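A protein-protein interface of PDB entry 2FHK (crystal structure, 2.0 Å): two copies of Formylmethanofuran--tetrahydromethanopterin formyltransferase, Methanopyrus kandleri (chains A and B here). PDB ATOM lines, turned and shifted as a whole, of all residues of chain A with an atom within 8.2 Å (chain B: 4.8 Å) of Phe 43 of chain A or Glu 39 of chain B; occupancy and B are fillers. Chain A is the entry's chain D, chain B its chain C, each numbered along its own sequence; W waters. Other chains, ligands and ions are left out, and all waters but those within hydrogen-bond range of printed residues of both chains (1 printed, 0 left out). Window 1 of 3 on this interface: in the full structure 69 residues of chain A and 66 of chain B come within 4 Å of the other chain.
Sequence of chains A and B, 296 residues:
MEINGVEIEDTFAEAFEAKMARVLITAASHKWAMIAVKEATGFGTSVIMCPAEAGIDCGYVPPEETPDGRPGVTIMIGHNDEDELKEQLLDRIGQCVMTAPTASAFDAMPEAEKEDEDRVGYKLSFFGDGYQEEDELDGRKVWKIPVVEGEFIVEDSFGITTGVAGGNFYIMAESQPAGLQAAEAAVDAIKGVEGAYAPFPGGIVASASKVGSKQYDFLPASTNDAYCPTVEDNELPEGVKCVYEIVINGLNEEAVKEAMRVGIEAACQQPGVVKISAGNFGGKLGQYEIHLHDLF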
ATOM      1  N   VAL A  37      24.346   0.558  18.448  1.00  0.00           N
ATOM      2  CA  VAL A  37      23.932   0.338  17.057  1.00  0.00           C
ATOM      3  C   VAL A  37      22.537   0.905  16.719  1.00  0.00           C
ATOM      4  O   VAL A  37      22.381   1.612  15.716  1.00  0.00           O
ATOM      5  CB  VAL A  37      24.024  -1.172  16.696  1.00  0.00           C
ATOM      6  CG1 VAL A  37      23.212  -1.503  15.454  1.00  0.00           C
ATOM      7  CG2 VAL A  37      25.482  -1.590  16.524  1.00  0.00           C
ATOM      8  N   LYS A  38      21.541   0.604  17.550  1.00  0.00           N
ATOM      9  CA  LYS A  38      20.166   1.073  17.323  1.00  0.00           C
ATOM     10  C   LYS A  38      20.067   2.593  17.391  1.00  0.00           C
ATOM     11  O   LYS A  38      19.352   3.216  16.601  1.00  0.00           O
ATOM     12  CB  LYS A  38      19.188   0.449  18.326  1.00  0.00           C
ATOM     13  CG  LYS A  38      19.084  -1.074  18.269  1.00  0.00           C
ATOM     14  CD  LYS A  38      17.982  -1.561  17.337  1.00  0.00           C
ATOM     15  CE  LYS A  38      18.471  -1.693  15.901  1.00  0.00           C
ATOM     16  NZ  LYS A  38      17.678  -2.693  15.128  1.00  0.00           N
ATOM     17  N   GLU A  39      20.789   3.184  18.337  1.00  0.00           N
ATOM     18  CA  GLU A  39      20.827   4.628  18.457  1.00  0.00           C
ATOM     19  C   GLU A  39      21.491   5.261  17.226  1.00  0.00           C
ATOM     20  O   GLU A  39      20.938   6.184  16.632  1.00  0.00           O
ATOM     21  CB  GLU A  39      21.527   5.049  19.757  1.00  0.00           C
ATOM     22  CG  GLU A  39      21.418   6.542  20.063  1.00  0.00           C
ATOM     23  CD  GLU A  39      19.991   7.011  20.284  1.00  0.00           C
ATOM     24  OE1 GLU A  39      19.632   8.124  19.816  1.00  0.00           O
ATOM     25  OE2 GLU A  39      19.215   6.282  20.938  1.00  0.00           O
ATOM     26  N   ALA A  40      22.654   4.737  16.843  1.00  0.00           N
ATOM     27  CA  ALA A  40      23.455   5.286  15.742  1.00  0.00           C
ATOM     28  C   ALA A  40      22.836   5.097  14.356  1.00  0.00           C
ATOM     29  O   ALA A  40      23.118   5.879  13.449  1.00  0.00           O
ATOM     30  CB  ALA A  40      24.859   4.708  15.771  1.00  0.00           C
ATOM     31  N   THR A  41      22.004   4.065  14.195  1.00  0.00           N
ATOM     32  CA  THR A  41      21.391   3.770  12.891  1.00  0.00           C
ATOM     33  C   THR A  41      19.927   4.202  12.763  1.00  0.00           C
ATOM     34  O   THR A  41      19.335   4.061  11.685  1.00  0.00           O
ATOM     35  CB  THR A  41      21.519   2.273  12.506  1.00  0.00           C
ATOM     36  OG1 THR A  41      20.823   1.459  13.466  1.00  0.00           O
ATOM     37  CG2 THR A  41      22.980   1.864  12.446  1.00  0.00           C
ATOM     38  N   GLY A  42      19.347   4.711  13.851  1.00  0.00           N
ATOM     39  CA  GLY A  42      17.965   5.187  13.852  1.00  0.00           C
ATOM     40  C   GLY A  42      17.848   6.532  13.162  1.00  0.00           C
ATOM     41  O   GLY A  42      18.865   7.138  12.816  1.00  0.00           O
ATOM     42  N   PHE A  43      16.613   6.992  12.957  1.00  0.00           N
ATOM     43  CA  PHE A  43      16.323   8.204  12.171  1.00  0.00           C
ATOM     44  C   PHE A  43      17.187   8.210  10.902  1.00  0.00           C
ATOM     45  O   PHE A  43      17.940   9.149  10.624  1.00  0.00           O
ATOM     46  CB  PHE A  43      16.493   9.477  13.027  1.00  0.00           C
ATOM     47  CG  PHE A  43      15.955  10.749  12.382  1.00  0.00           C
ATOM     48  CD1 PHE A  43      14.844  10.723  11.532  1.00  0.00           C
ATOM     49  CD2 PHE A  43      16.555  11.981  12.657  1.00  0.00           C
ATOM     50  CE1 PHE A  43      14.356  11.900  10.949  1.00  0.00           C
ATOM     51  CE2 PHE A  43      16.064  13.167  12.090  1.00  0.00           C
ATOM     52  CZ  PHE A  43      14.963  13.121  11.229  1.00  0.00           C
ATOM     53  N   GLY A  44      17.090   7.119  10.150  1.00  0.00           N
ATOM     54  CA  GLY A  44      17.943   6.914   8.991  1.00  0.00           C
ATOM     55  C   GLY A  44      17.359   5.904   8.029  1.00  0.00           C
ATOM     56  O   GLY A  44      18.000   4.898   7.712  1.00  0.00           O
ATOM     57  N   THR A  45      16.133   6.159   7.583  1.00  0.00           N
ATOM     58  CA  THR A  45      15.451   5.269   6.645  1.00  0.00           C
ATOM     59  C   THR A  45      15.679   5.719   5.207  1.00  0.00           C
ATOM     60  O   THR A  45      15.882   4.898   4.315  1.00  0.00           O
ATOM     61  CB  THR A  45      13.925   5.203   6.900  1.00  0.00           C
ATOM     62  OG1 THR A  45      13.342   6.502   6.724  1.00  0.00           O
ATOM     63  CG2 THR A  45      13.622   4.696   8.312  1.00  0.00           C
ATOM     64  N   SER A  46      15.651   7.034   4.997  1.00  0.00           N
ATOM     65  CA  SER A  46      15.641   7.616   3.663  1.00  0.00           C
ATOM     66  C   SER A  46      16.183   9.033   3.729  1.00  0.00           C
ATOM     67  O   SER A  46      15.855   9.765   4.649  1.00  0.00           O
ATOM     68  CB  SER A  46      14.206   7.646   3.136  1.00  0.00           C
ATOM     69  OG  SER A  46      14.113   8.414   1.956  1.00  0.00           O
ATOM     70  N   VAL A  47      17.001   9.420   2.753  1.00  0.00           N
ATOM     71  CA  VAL A  47      17.517  10.795   2.689  1.00  0.00           C
ATOM     72  C   VAL A  47      16.461  11.824   2.250  1.00  0.00           C
ATOM     73  O   VAL A  47      16.741  13.034   2.219  1.00  0.00           O
ATOM     74  CB  VAL A  47      18.778  10.921   1.789  1.00  0.00           C
ATOM     75  CG1 VAL A  47      19.957  10.160   2.392  1.00  0.00           C
ATOM     76  CG2 VAL A  47      18.481  10.467   0.369  1.00  0.00           C
ATOM     77  N   MET A  49      13.702  12.635   3.967  1.00  0.00           N
ATOM     78  CA  MET A  49      13.484  13.470   5.158  1.00  0.00           C
ATOM     79  C   MET A  49      14.317  13.088   6.396  1.00  0.00           C
ATOM     80  O   MET A  49      14.201  13.739   7.441  1.00  0.00           O
ATOM     81  CB  MET A  49      11.993  13.555   5.516  1.00  0.00           C
ATOM     82  CG  MET A  49      11.110  14.252   4.462  1.00  0.00           C
ATOM     83  SD  MET A  49       9.569  14.926   5.123  1.00  0.00           S
ATOM     84  CE  MET A  49       8.859  13.489   5.950  1.00  0.00           C
ATOM     85  N   CYS A  50      15.150  12.048   6.277  1.00  0.00           N
ATOM     86  CA  CYS A  50      16.140  11.707   7.315  1.00  0.00           C
ATOM     87  C   CYS A  50      17.536  12.212   6.930  1.00  0.00           C
ATOM     88  O   CYS A  50      17.827  12.393   5.747  1.00  0.00           O
ATOM     89  CB  CYS A  50      16.215  10.193   7.535  1.00  0.00           C
ATOM     90  SG  CYS A  50      14.677   9.381   7.932  1.00  0.00           S
ATOM     91  N   PRO A  51      18.419  12.416   7.928  1.00  0.00           N
ATOM     92  CA  PRO A  51      19.777  12.885   7.655  1.00  0.00           C
ATOM     93  C   PRO A  51      20.700  11.870   6.951  1.00  0.00           C
ATOM     94  O   PRO A  51      21.727  12.268   6.388  1.00  0.00           O
ATOM     95  CB  PRO A  51      20.314  13.233   9.055  1.00  0.00           C
ATOM     96  CG  PRO A  51      19.118  13.290   9.949  1.00  0.00           C
ATOM     97  CD  PRO A  51      18.192  12.274   9.376  1.00  0.00           C
ATOM     98  N   ALA A  52      20.344  10.586   6.984  1.00  0.00           N
ATOM     99  CA  ALA A  52      21.139   9.532   6.344  1.00  0.00           C
ATOM    100  C   ALA A  52      20.326   8.256   6.150  1.00  0.00           C
ATOM    101  O   ALA A  52      19.192   8.165   6.607  1.00  0.00           O
ATOM    102  CB  ALA A  52      22.402   9.229   7.169  1.00  0.00           C
ATOM    103  N   GLU A  53      20.915   7.283   5.457  1.00  0.00           N
ATOM    104  CA  GLU A  53      20.345   5.947   5.330  1.00  0.00           C
ATOM    105  C   GLU A  53      21.305   4.984   6.011  1.00  0.00           C
ATOM    106  O   GLU A  53      22.441   4.806   5.562  1.00  0.00           O
ATOM    107  CB  GLU A  53      20.137   5.570   3.861  1.00  0.00           C
ATOM    108  CG  GLU A  53      18.950   6.257   3.217  1.00  0.00           C
ATOM    109  CD  GLU A  53      18.931   6.145   1.694  1.00  0.00           C
ATOM    110  OE1 GLU A  53      19.719   5.358   1.132  1.00  0.00           O
ATOM    111  OE2 GLU A  53      18.110   6.837   1.055  1.00  0.00           O
ATOM    112  N   ALA A  54      20.850   4.365   7.096  1.00  0.00           N
ATOM    113  CA  ALA A  54      21.728   3.576   7.951  1.00  0.00           C
ATOM    114  C   ALA A  54      21.057   2.288   8.405  1.00  0.00           C
ATOM    115  O   ALA A  54      19.827   2.199   8.418  1.00  0.00           O
ATOM    116  CB  ALA A  54      22.161   4.393   9.163  1.00  0.00           C
ATOM    117  N   GLY A  55      21.865   1.304   8.794  1.00  0.00           N
ATOM    118  CA  GLY A  55      21.343   0.019   9.225  1.00  0.00           C
ATOM    119  C   GLY A  55      22.426  -0.951   9.648  1.00  0.00           C
ATOM    120  O   GLY A  55      23.614  -0.749   9.386  1.00  0.00           O
ATOM    121  N   GLN A  88      27.527  12.977   8.882  1.00  0.00           N
ATOM    122  CA  GLN A  88      26.697  11.951   9.529  1.00  0.00           C
ATOM    123  C   GLN A  88      27.526  10.941  10.326  1.00  0.00           C
ATOM    124  O   GLN A  88      27.113  10.493  11.403  1.00  0.00           O
ATOM    125  CB  GLN A  88      25.831  11.225   8.493  1.00  0.00           C
ATOM    126  CG  GLN A  88      24.645  12.039   7.989  1.00  0.00           C
ATOM    127  CD  GLN A  88      23.702  12.414   9.108  1.00  0.00           C
ATOM    128  OE1 GLN A  88      23.066  11.546   9.718  1.00  0.00           O
ATOM    129  NE2 GLN A  88      23.616  13.714   9.398  1.00  0.00           N
ATOM    130  N   ARG A  92      26.860  10.716  14.236  1.00  0.00           N
ATOM    131  CA  ARG A  92      26.348   9.423  14.731  1.00  0.00           C
ATOM    132  C   ARG A  92      27.333   8.672  15.625  1.00  0.00           C
ATOM    133  O   ARG A  92      26.938   8.106  16.641  1.00  0.00           O
ATOM    134  CB  ARG A  92      25.855   8.550  13.575  1.00  0.00           C
ATOM    135  CG  ARG A  92      24.524   9.037  12.994  1.00  0.00           C
ATOM    136  CD  ARG A  92      24.221   8.419  11.639  1.00  0.00           C
ATOM    137  NE  ARG A  92      23.073   9.067  10.993  1.00  0.00           N
ATOM    138  CZ  ARG A  92      21.806   8.686  11.140  1.00  0.00           C
ATOM    139  NH1 ARG A  92      20.844   9.338  10.502  1.00  0.00           N
ATOM    140  NH2 ARG A  92      21.498   7.659  11.924  1.00  0.00           N
ATOM    141  N   ALA A 198      19.193  -3.019   5.050  1.00  0.00           N
ATOM    142  CA  ALA A 198      17.853  -2.535   4.745  1.00  0.00           C
ATOM    143  C   ALA A 198      17.495  -1.421   5.729  1.00  0.00           C
ATOM    144  O   ALA A 198      17.171  -1.702   6.886  1.00  0.00           O
ATOM    145  CB  ALA A 198      16.846  -3.675   4.823  1.00  0.00           C
ATOM    146  N   PRO A 199      17.576  -0.155   5.278  1.00  0.00           N
ATOM    147  CA  PRO A 199      17.470   1.004   6.174  1.00  0.00           C
ATOM    148  C   PRO A 199      16.101   1.296   6.800  1.00  0.00           C
ATOM    149  O   PRO A 199      16.049   1.946   7.838  1.00  0.00           O
ATOM    150  CB  PRO A 199      17.908   2.172   5.288  1.00  0.00           C
ATOM    151  CG  PRO A 199      17.550   1.744   3.913  1.00  0.00           C
ATOM    152  CD  PRO A 199      17.805   0.265   3.881  1.00  0.00           C
ATOM    153  N   PHE A 200      15.013   0.839   6.189  1.00  0.00           N
ATOM    154  CA  PHE A 200      13.663   1.106   6.718  1.00  0.00           C
ATOM    155  C   PHE A 200      13.350   0.331   8.017  1.00  0.00           C
ATOM    156  O   PHE A 200      14.100  -0.573   8.388  1.00  0.00           O
ATOM    157  CB  PHE A 200      12.609   0.911   5.620  1.00  0.00           C
ATOM    158  CG  PHE A 200      12.641   1.999   4.578  1.00  0.00           C
ATOM    159  CD1 PHE A 200      13.488   1.906   3.480  1.00  0.00           C
ATOM    160  CD2 PHE A 200      11.859   3.134   4.725  1.00  0.00           C
ATOM    161  CE1 PHE A 200      13.535   2.924   2.520  1.00  0.00           C
ATOM    162  CE2 PHE A 200      11.896   4.163   3.779  1.00  0.00           C
ATOM    163  CZ  PHE A 200      12.734   4.053   2.672  1.00  0.00           C
ATOM    164  N   PRO A 201      12.274   0.715   8.733  1.00  0.00           N
ATOM    165  CA  PRO A 201      12.000   0.072  10.028  1.00  0.00           C
ATOM    166  C   PRO A 201      11.756  -1.434   9.904  1.00  0.00           C
ATOM    167  O   PRO A 201      10.837  -1.864   9.205  1.00  0.00           O
ATOM    168  CB  PRO A 201      10.744   0.799  10.529  1.00  0.00           C
ATOM    169  CG  PRO A 201      10.716   2.094   9.769  1.00  0.00           C
ATOM    170  CD  PRO A 201      11.275   1.760   8.421  1.00  0.00           C
ATOM    171  N   GLY A 202      12.592  -2.217  10.576  1.00  0.00           N
ATOM    172  CA  GLY A 202      12.573  -3.685  10.451  1.00  0.00           C
ATOM    173  C   GLY A 202      12.941  -4.159   9.053  1.00  0.00           C
ATOM    174  O   GLY A 202      12.758  -5.338   8.721  1.00  0.00           O
ATOM    175  N   GLY A 203      13.459  -3.232   8.245  1.00  0.00           N
ATOM    176  CA  GLY A 203      13.894  -3.497   6.869  1.00  0.00           C
ATOM    177  C   GLY A 203      12.824  -3.296   5.808  1.00  0.00           C
ATOM    178  O   GLY A 203      13.094  -3.428   4.609  1.00  0.00           O
ATOM    179  N   ILE B  35       9.577  -1.664  16.845  1.00  0.00           N
ATOM    180  CA  ILE B  35      10.284  -1.445  15.586  1.00  0.00           C
ATOM    181  C   ILE B  35      10.187   0.019  15.136  1.00  0.00           C
ATOM    182  O   ILE B  35      11.207   0.654  14.867  1.00  0.00           O
ATOM    183  CB  ILE B  35       9.781  -2.411  14.465  1.00  0.00           C
ATOM    184  CG1 ILE B  35      10.190  -3.871  14.763  1.00  0.00           C
ATOM    185  CG2 ILE B  35      10.254  -1.969  13.083  1.00  0.00           C
ATOM    186  CD1 ILE B  35      11.693  -4.131  14.784  1.00  0.00           C
ATOM    187  N   ALA B  36       8.963   0.543  15.065  1.00  0.00           N
ATOM    188  CA  ALA B  36       8.737   1.939  14.691  1.00  0.00           C
ATOM    189  C   ALA B  36       9.405   2.871  15.700  1.00  0.00           C
ATOM    190  O   ALA B  36      10.106   3.814  15.321  1.00  0.00           O
ATOM    191  CB  ALA B  36       7.236   2.234  14.586  1.00  0.00           C
ATOM    192  N   VAL B  37       9.188   2.579  16.978  1.00  0.00           N
ATOM    193  CA  VAL B  37       9.723   3.352  18.100  1.00  0.00           C
ATOM    194  C   VAL B  37      11.251   3.529  18.059  1.00  0.00           C
ATOM    195  O   VAL B  37      11.754   4.658  18.174  1.00  0.00           O
ATOM    196  CB  VAL B  37       9.256   2.733  19.453  1.00  0.00           C
ATOM    197  CG1 VAL B  37      10.085   3.249  20.615  1.00  0.00           C
ATOM    198  CG2 VAL B  37       7.783   3.026  19.675  1.00  0.00           C
ATOM    199  N   LYS B  38      11.980   2.424  17.891  1.00  0.00           N
ATOM    200  CA  LYS B  38      13.447   2.465  17.878  1.00  0.00           C
ATOM    201  C   LYS B  38      13.968   3.297  16.708  1.00  0.00           C
ATOM    202  O   LYS B  38      14.938   4.041  16.845  1.00  0.00           O
ATOM    203  CB  LYS B  38      14.042   1.053  17.834  1.00  0.00           C
ATOM    204  CG  LYS B  38      13.714   0.169  19.040  1.00  0.00           C
ATOM    205  CD  LYS B  38      14.742   0.277  20.169  1.00  0.00           C
ATOM    206  CE  LYS B  38      14.432   1.425  21.123  1.00  0.00           C
ATOM    207  NZ  LYS B  38      14.996   1.195  22.484  1.00  0.00           N
ATOM    208  N   GLU B  39      13.314   3.172  15.555  1.00  0.00           N
ATOM    209  CA  GLU B  39      13.678   3.967  14.391  1.00  0.00           C
ATOM    210  C   GLU B  39      13.398   5.454  14.621  1.00  0.00           C
ATOM    211  O   GLU B  39      14.261   6.292  14.364  1.00  0.00           O
ATOM    212  CB  GLU B  39      12.962   3.458  13.137  1.00  0.00           C
ATOM    213  CG  GLU B  39      13.464   4.081  11.827  1.00  0.00           C
ATOM    214  CD  GLU B  39      14.922   3.773  11.515  1.00  0.00           C
ATOM    215  OE1 GLU B  39      15.637   4.664  10.993  1.00  0.00           O
ATOM    216  OE2 GLU B  39      15.373   2.632  11.770  1.00  0.00           O
ATOM    217  N   ALA B  40      12.202   5.767  15.114  1.00  0.00           N
ATOM    218  CA  ALA B  40      11.752   7.156  15.286  1.00  0.00           C
ATOM    219  C   ALA B  40      12.481   7.907  16.402  1.00  0.00           C
ATOM    220  O   ALA B  40      12.572   9.134  16.357  1.00  0.00           O
ATOM    221  CB  ALA B  40      10.242   7.201  15.523  1.00  0.00           C
ATOM    222  N   THR B  41      12.992   7.177  17.397  1.00  0.00           N
ATOM    223  CA  THR B  41      13.661   7.811  18.543  1.00  0.00           C
ATOM    224  C   THR B  41      15.191   7.758  18.468  1.00  0.00           C
ATOM    225  O   THR B  41      15.874   8.330  19.325  1.00  0.00           O
ATOM    226  CB  THR B  41      13.182   7.229  19.910  1.00  0.00           C
ATOM    227  OG1 THR B  41      13.491   5.833  19.986  1.00  0.00           O
ATOM    228  CG2 THR B  41      11.682   7.430  20.088  1.00  0.00           C
ATOM    229  N   GLY B  42      15.723   7.071  17.455  1.00  0.00           N
ATOM    230  CA  GLY B  42      17.171   6.928  17.285  1.00  0.00           C
ATOM    231  C   GLY B  42      17.790   8.210  16.761  1.00  0.00           C
ATOM    232  O   GLY B  42      17.067   9.145  16.408  1.00  0.00           O
ATOM    233  N   PHE B  43      19.122   8.254  16.720  1.00  0.00           N
ATOM    234  CA  PHE B  43      19.882   9.467  16.374  1.00  0.00           C
ATOM    235  C   PHE B  43      19.244  10.678  17.068  1.00  0.00           C
ATOM    236  O   PHE B  43      18.867  11.662  16.431  1.00  0.00           O
ATOM    237  CB  PHE B  43      19.964   9.631  14.843  1.00  0.00           C
ATOM    238  CG  PHE B  43      20.920  10.713  14.372  1.00  0.00           C
ATOM    239  CD1 PHE B  43      22.086  11.001  15.070  1.00  0.00           C
ATOM    240  CD2 PHE B  43      20.656  11.420  13.201  1.00  0.00           C
ATOM    241  CE1 PHE B  43      22.970  12.004  14.623  1.00  0.00           C
ATOM    242  CE2 PHE B  43      21.536  12.414  12.742  1.00  0.00           C
ATOM    243  CZ  PHE B  43      22.694  12.703  13.459  1.00  0.00           C
ATOM    244  N   PRO B  51      19.666  15.763  15.669  1.00  0.00           N
ATOM    245  CA  PRO B  51      18.547  16.635  15.300  1.00  0.00           C
ATOM    246  C   PRO B  51      17.484  16.838  16.391  1.00  0.00           C
ATOM    247  O   PRO B  51      16.690  17.781  16.301  1.00  0.00           O
ATOM    248  CB  PRO B  51      17.937  15.929  14.080  1.00  0.00           C
ATOM    249  CG  PRO B  51      18.965  14.933  13.624  1.00  0.00           C
ATOM    250  CD  PRO B  51      19.651  14.515  14.884  1.00  0.00           C
ATOM    251  N   GLN B  88      11.079  18.036  13.392  1.00  0.00           N
ATOM    252  CA  GLN B  88      11.463  16.698  13.857  1.00  0.00           C
ATOM    253  C   GLN B  88      10.285  15.754  13.993  1.00  0.00           C
ATOM    254  O   GLN B  88      10.411  14.560  13.700  1.00  0.00           O
ATOM    255  CB  GLN B  88      12.223  16.769  15.182  1.00  0.00           C
ATOM    256  CG  GLN B  88      13.648  17.279  15.043  1.00  0.00           C
ATOM    257  CD  GLN B  88      14.488  16.389  14.168  1.00  0.00           C
ATOM    258  OE1 GLN B  88      14.756  15.229  14.509  1.00  0.00           O
ATOM    259  NE2 GLN B  88      14.914  16.922  13.020  1.00  0.00           N
ATOM    260  N   ASP B  91       9.416  14.779  10.381  1.00  0.00           N
ATOM    261  CA  ASP B  91      10.444  13.917   9.797  1.00  0.00           C
ATOM    262  C   ASP B  91      10.429  12.510  10.401  1.00  0.00           C
ATOM    263  O   ASP B  91      10.505  11.527   9.677  1.00  0.00           O
ATOM    264  CB  ASP B  91      11.834  14.542   9.978  1.00  0.00           C
ATOM    265  CG  ASP B  91      12.053  15.775   9.104  1.00  0.00           C
ATOM    266  OD1 ASP B  91      11.185  16.093   8.263  1.00  0.00           O
ATOM    267  OD2 ASP B  91      13.110  16.426   9.267  1.00  0.00           O
ATOM    268  N   ARG B  92      10.330  12.432  11.723  1.00  0.00           N
ATOM    269  CA  ARG B  92      10.360  11.157  12.439  1.00  0.00           C
ATOM    270  C   ARG B  92       9.069  10.344  12.289  1.00  0.00           C
ATOM    271  O   ARG B  92       9.125   9.137  12.084  1.00  0.00           O
ATOM    272  CB  ARG B  92      10.724  11.382  13.907  1.00  0.00           C
ATOM    273  CG  ARG B  92      12.210  11.740  14.091  1.00  0.00           C
ATOM    274  CD  ARG B  92      12.515  12.248  15.482  1.00  0.00           C
ATOM    275  NE  ARG B  92      13.870  12.790  15.557  1.00  0.00           N
ATOM    276  CZ  ARG B  92      14.939  12.103  15.954  1.00  0.00           C
ATOM    277  NH1 ARG B  92      16.128  12.690  15.991  1.00  0.00           N
ATOM    278  NH2 ARG B  92      14.817  10.833  16.330  1.00  0.00           N
ATOM    279  N   CYS B  96       9.748   7.337   9.732  1.00  0.00           N
ATOM    280  CA  CYS B  96      10.058   6.217  10.620  1.00  0.00           C
ATOM    281  C   CYS B  96       8.830   5.511  11.188  1.00  0.00           C
ATOM    282  O   CYS B  96       8.916   4.349  11.606  1.00  0.00           O
ATOM    283  CB  CYS B  96      10.957   6.690  11.766  1.00  0.00           C
ATOM    284  SG  CYS B  96      12.420   7.611  11.254  1.00  0.00           S
HETATM  285  O   HOH W   1      18.048   0.807  12.086  1.00  0.00           O
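O of Glu 39 of chain B is in hydrogen-bond range of N of Phe 43 of chain A, 2.8 Å away. The side-chain carboxylate of Glu 39 of chain B is in hydrogen-bond range of the backbone NH of Gly 44 of chain A (3.0 Å). The backbone NH of Phe 43 of chain B sits at hydrogen-bond distance from the backbone carbonyl oxygen of Glu 39 of chain A, 2.8 Å away. The backbone carbonyl oxygen (O) of Met 49 of chain A lies close to the side-chain carboxylate (OD2) of Asp 91 of chain B, at 3.4 Å.
O of Gly 42 of chain B is in hydrogen-bond range of NH2 of Arg 92 of chain B, at 2.8 Å. The side-chain hydroxyl (OG1) of Thr 41 of chain A lies within hydrogen-bond range of the backbone carbonyl oxygen (O) of Val 37 of chain A, at 2.7 Å. The backbone carbonyl oxygen (O) of Gly 42 of chain A sits at hydrogen-bond distance from the guanidinium group (NH2) of Arg 92 of chain A (2.8 Å). The backbone carbonyl oxygen (O) of Phe 43 of chain A lies within hydrogen-bond range of the guanidinium group (NH1) of Arg 92 of chain A, 2.9 Å away. The backbone carbonyl oxygen (O) of Gly 44 of chain A sits at hydrogen-bond distance from the backbone NH (N) of Ala 54 of chain A, at 3.0 Å. OG1 of Thr 45 of chain A is in hydrogen-bond range of SG of Cys 50 of chain A (3.4 Å).
Thr 41 of chain A touches Glu 39 of chain B. Gly 42 of chain A touches Glu 39 of chain B. Gly 42 of chain A touches Gly 42 of chain B. CB of Phe 43 of chain A touches O of Gly 42 of chain B, 3.4 Å away. Phe 43 of chain B touches Phe 43 of chain A. Phe 43 of chain A touches Asp 91 of chain B. Thr 45 of chain A touches Glu 39 of chain B (CG2 to OE1, 3.4 Å). Pro 201 of chain A touches Ile 35 of chain B. CG of Pro 201 of chain A touches CG of Glu 39 of chain B (3.97 Å). Ile 35 of chain B touches Gly 202 of chain A (CG2 to N, 3.4 Å).
Of chain A, only Thr 41, Gly 42, Phe 43, Gly 44, Thr 45 and Pro 201 come within 4 Å of Glu 39 of chain B. Of the printed residues of chain B, Thr 41 of chain A touches Glu 39. Printed residues of chain B within 4 Å of Arg 92 of chain A: Phe 43. Of the printed residues of chain B, Pro 51 of chain A touches Phe 43 (3.8 Å). Printed residues of chain A within 4 Å of Ile 35 of chain B: Pro 201 (3.6 Å) and Gly 202 (3.4 Å). Of the printed residues of chain B, Thr 45 of chain A touches Glu 39. Ala 36 of chain B touches none of the printed residues of chain A. Pro 199 of chain A touches none of the printed residues of chain B. The nearest printed residue of chain B that does not touch Phe 43 of chain A is Ala 40 of chain B (5.1 Å).
Hydrophobic or aromatic side chains of chain B within 4 Å of the printed part of chain A: Ile 35, Phe 43 and Pro 51. Among the printed residues, 25 pairs touch across the chains. Among the printed residues, no Asp or Glu carboxylate lies within 4 Å of a Lys or Arg side-chain nitrogen of the other chain.
Glu 39 of chain A touches Thr 41 of chain B, and with the chains exchanged Thr 41 of chain A touches Glu 39 of chain B. Gly 42 of chain B touches its own counterpart, Gly 42 of chain A. Phe 43 of chain B touches its own counterpart, Phe 43 of chain A. Phe 43 of chain A touches Pro 51 of chain B, and with the chains exchanged Pro 51 of chain A touches Phe 43 of chain B. Of the 25 pairs that touch across the chains among the printed residues, 16 have their exchanged pair printed and touching as well.
Water W1 lies within hydrogen-bond range of OG1 of Thr 41 of chain A (3.2 Å) and OE2 of Glu 39 of chain B (3.3 Å).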
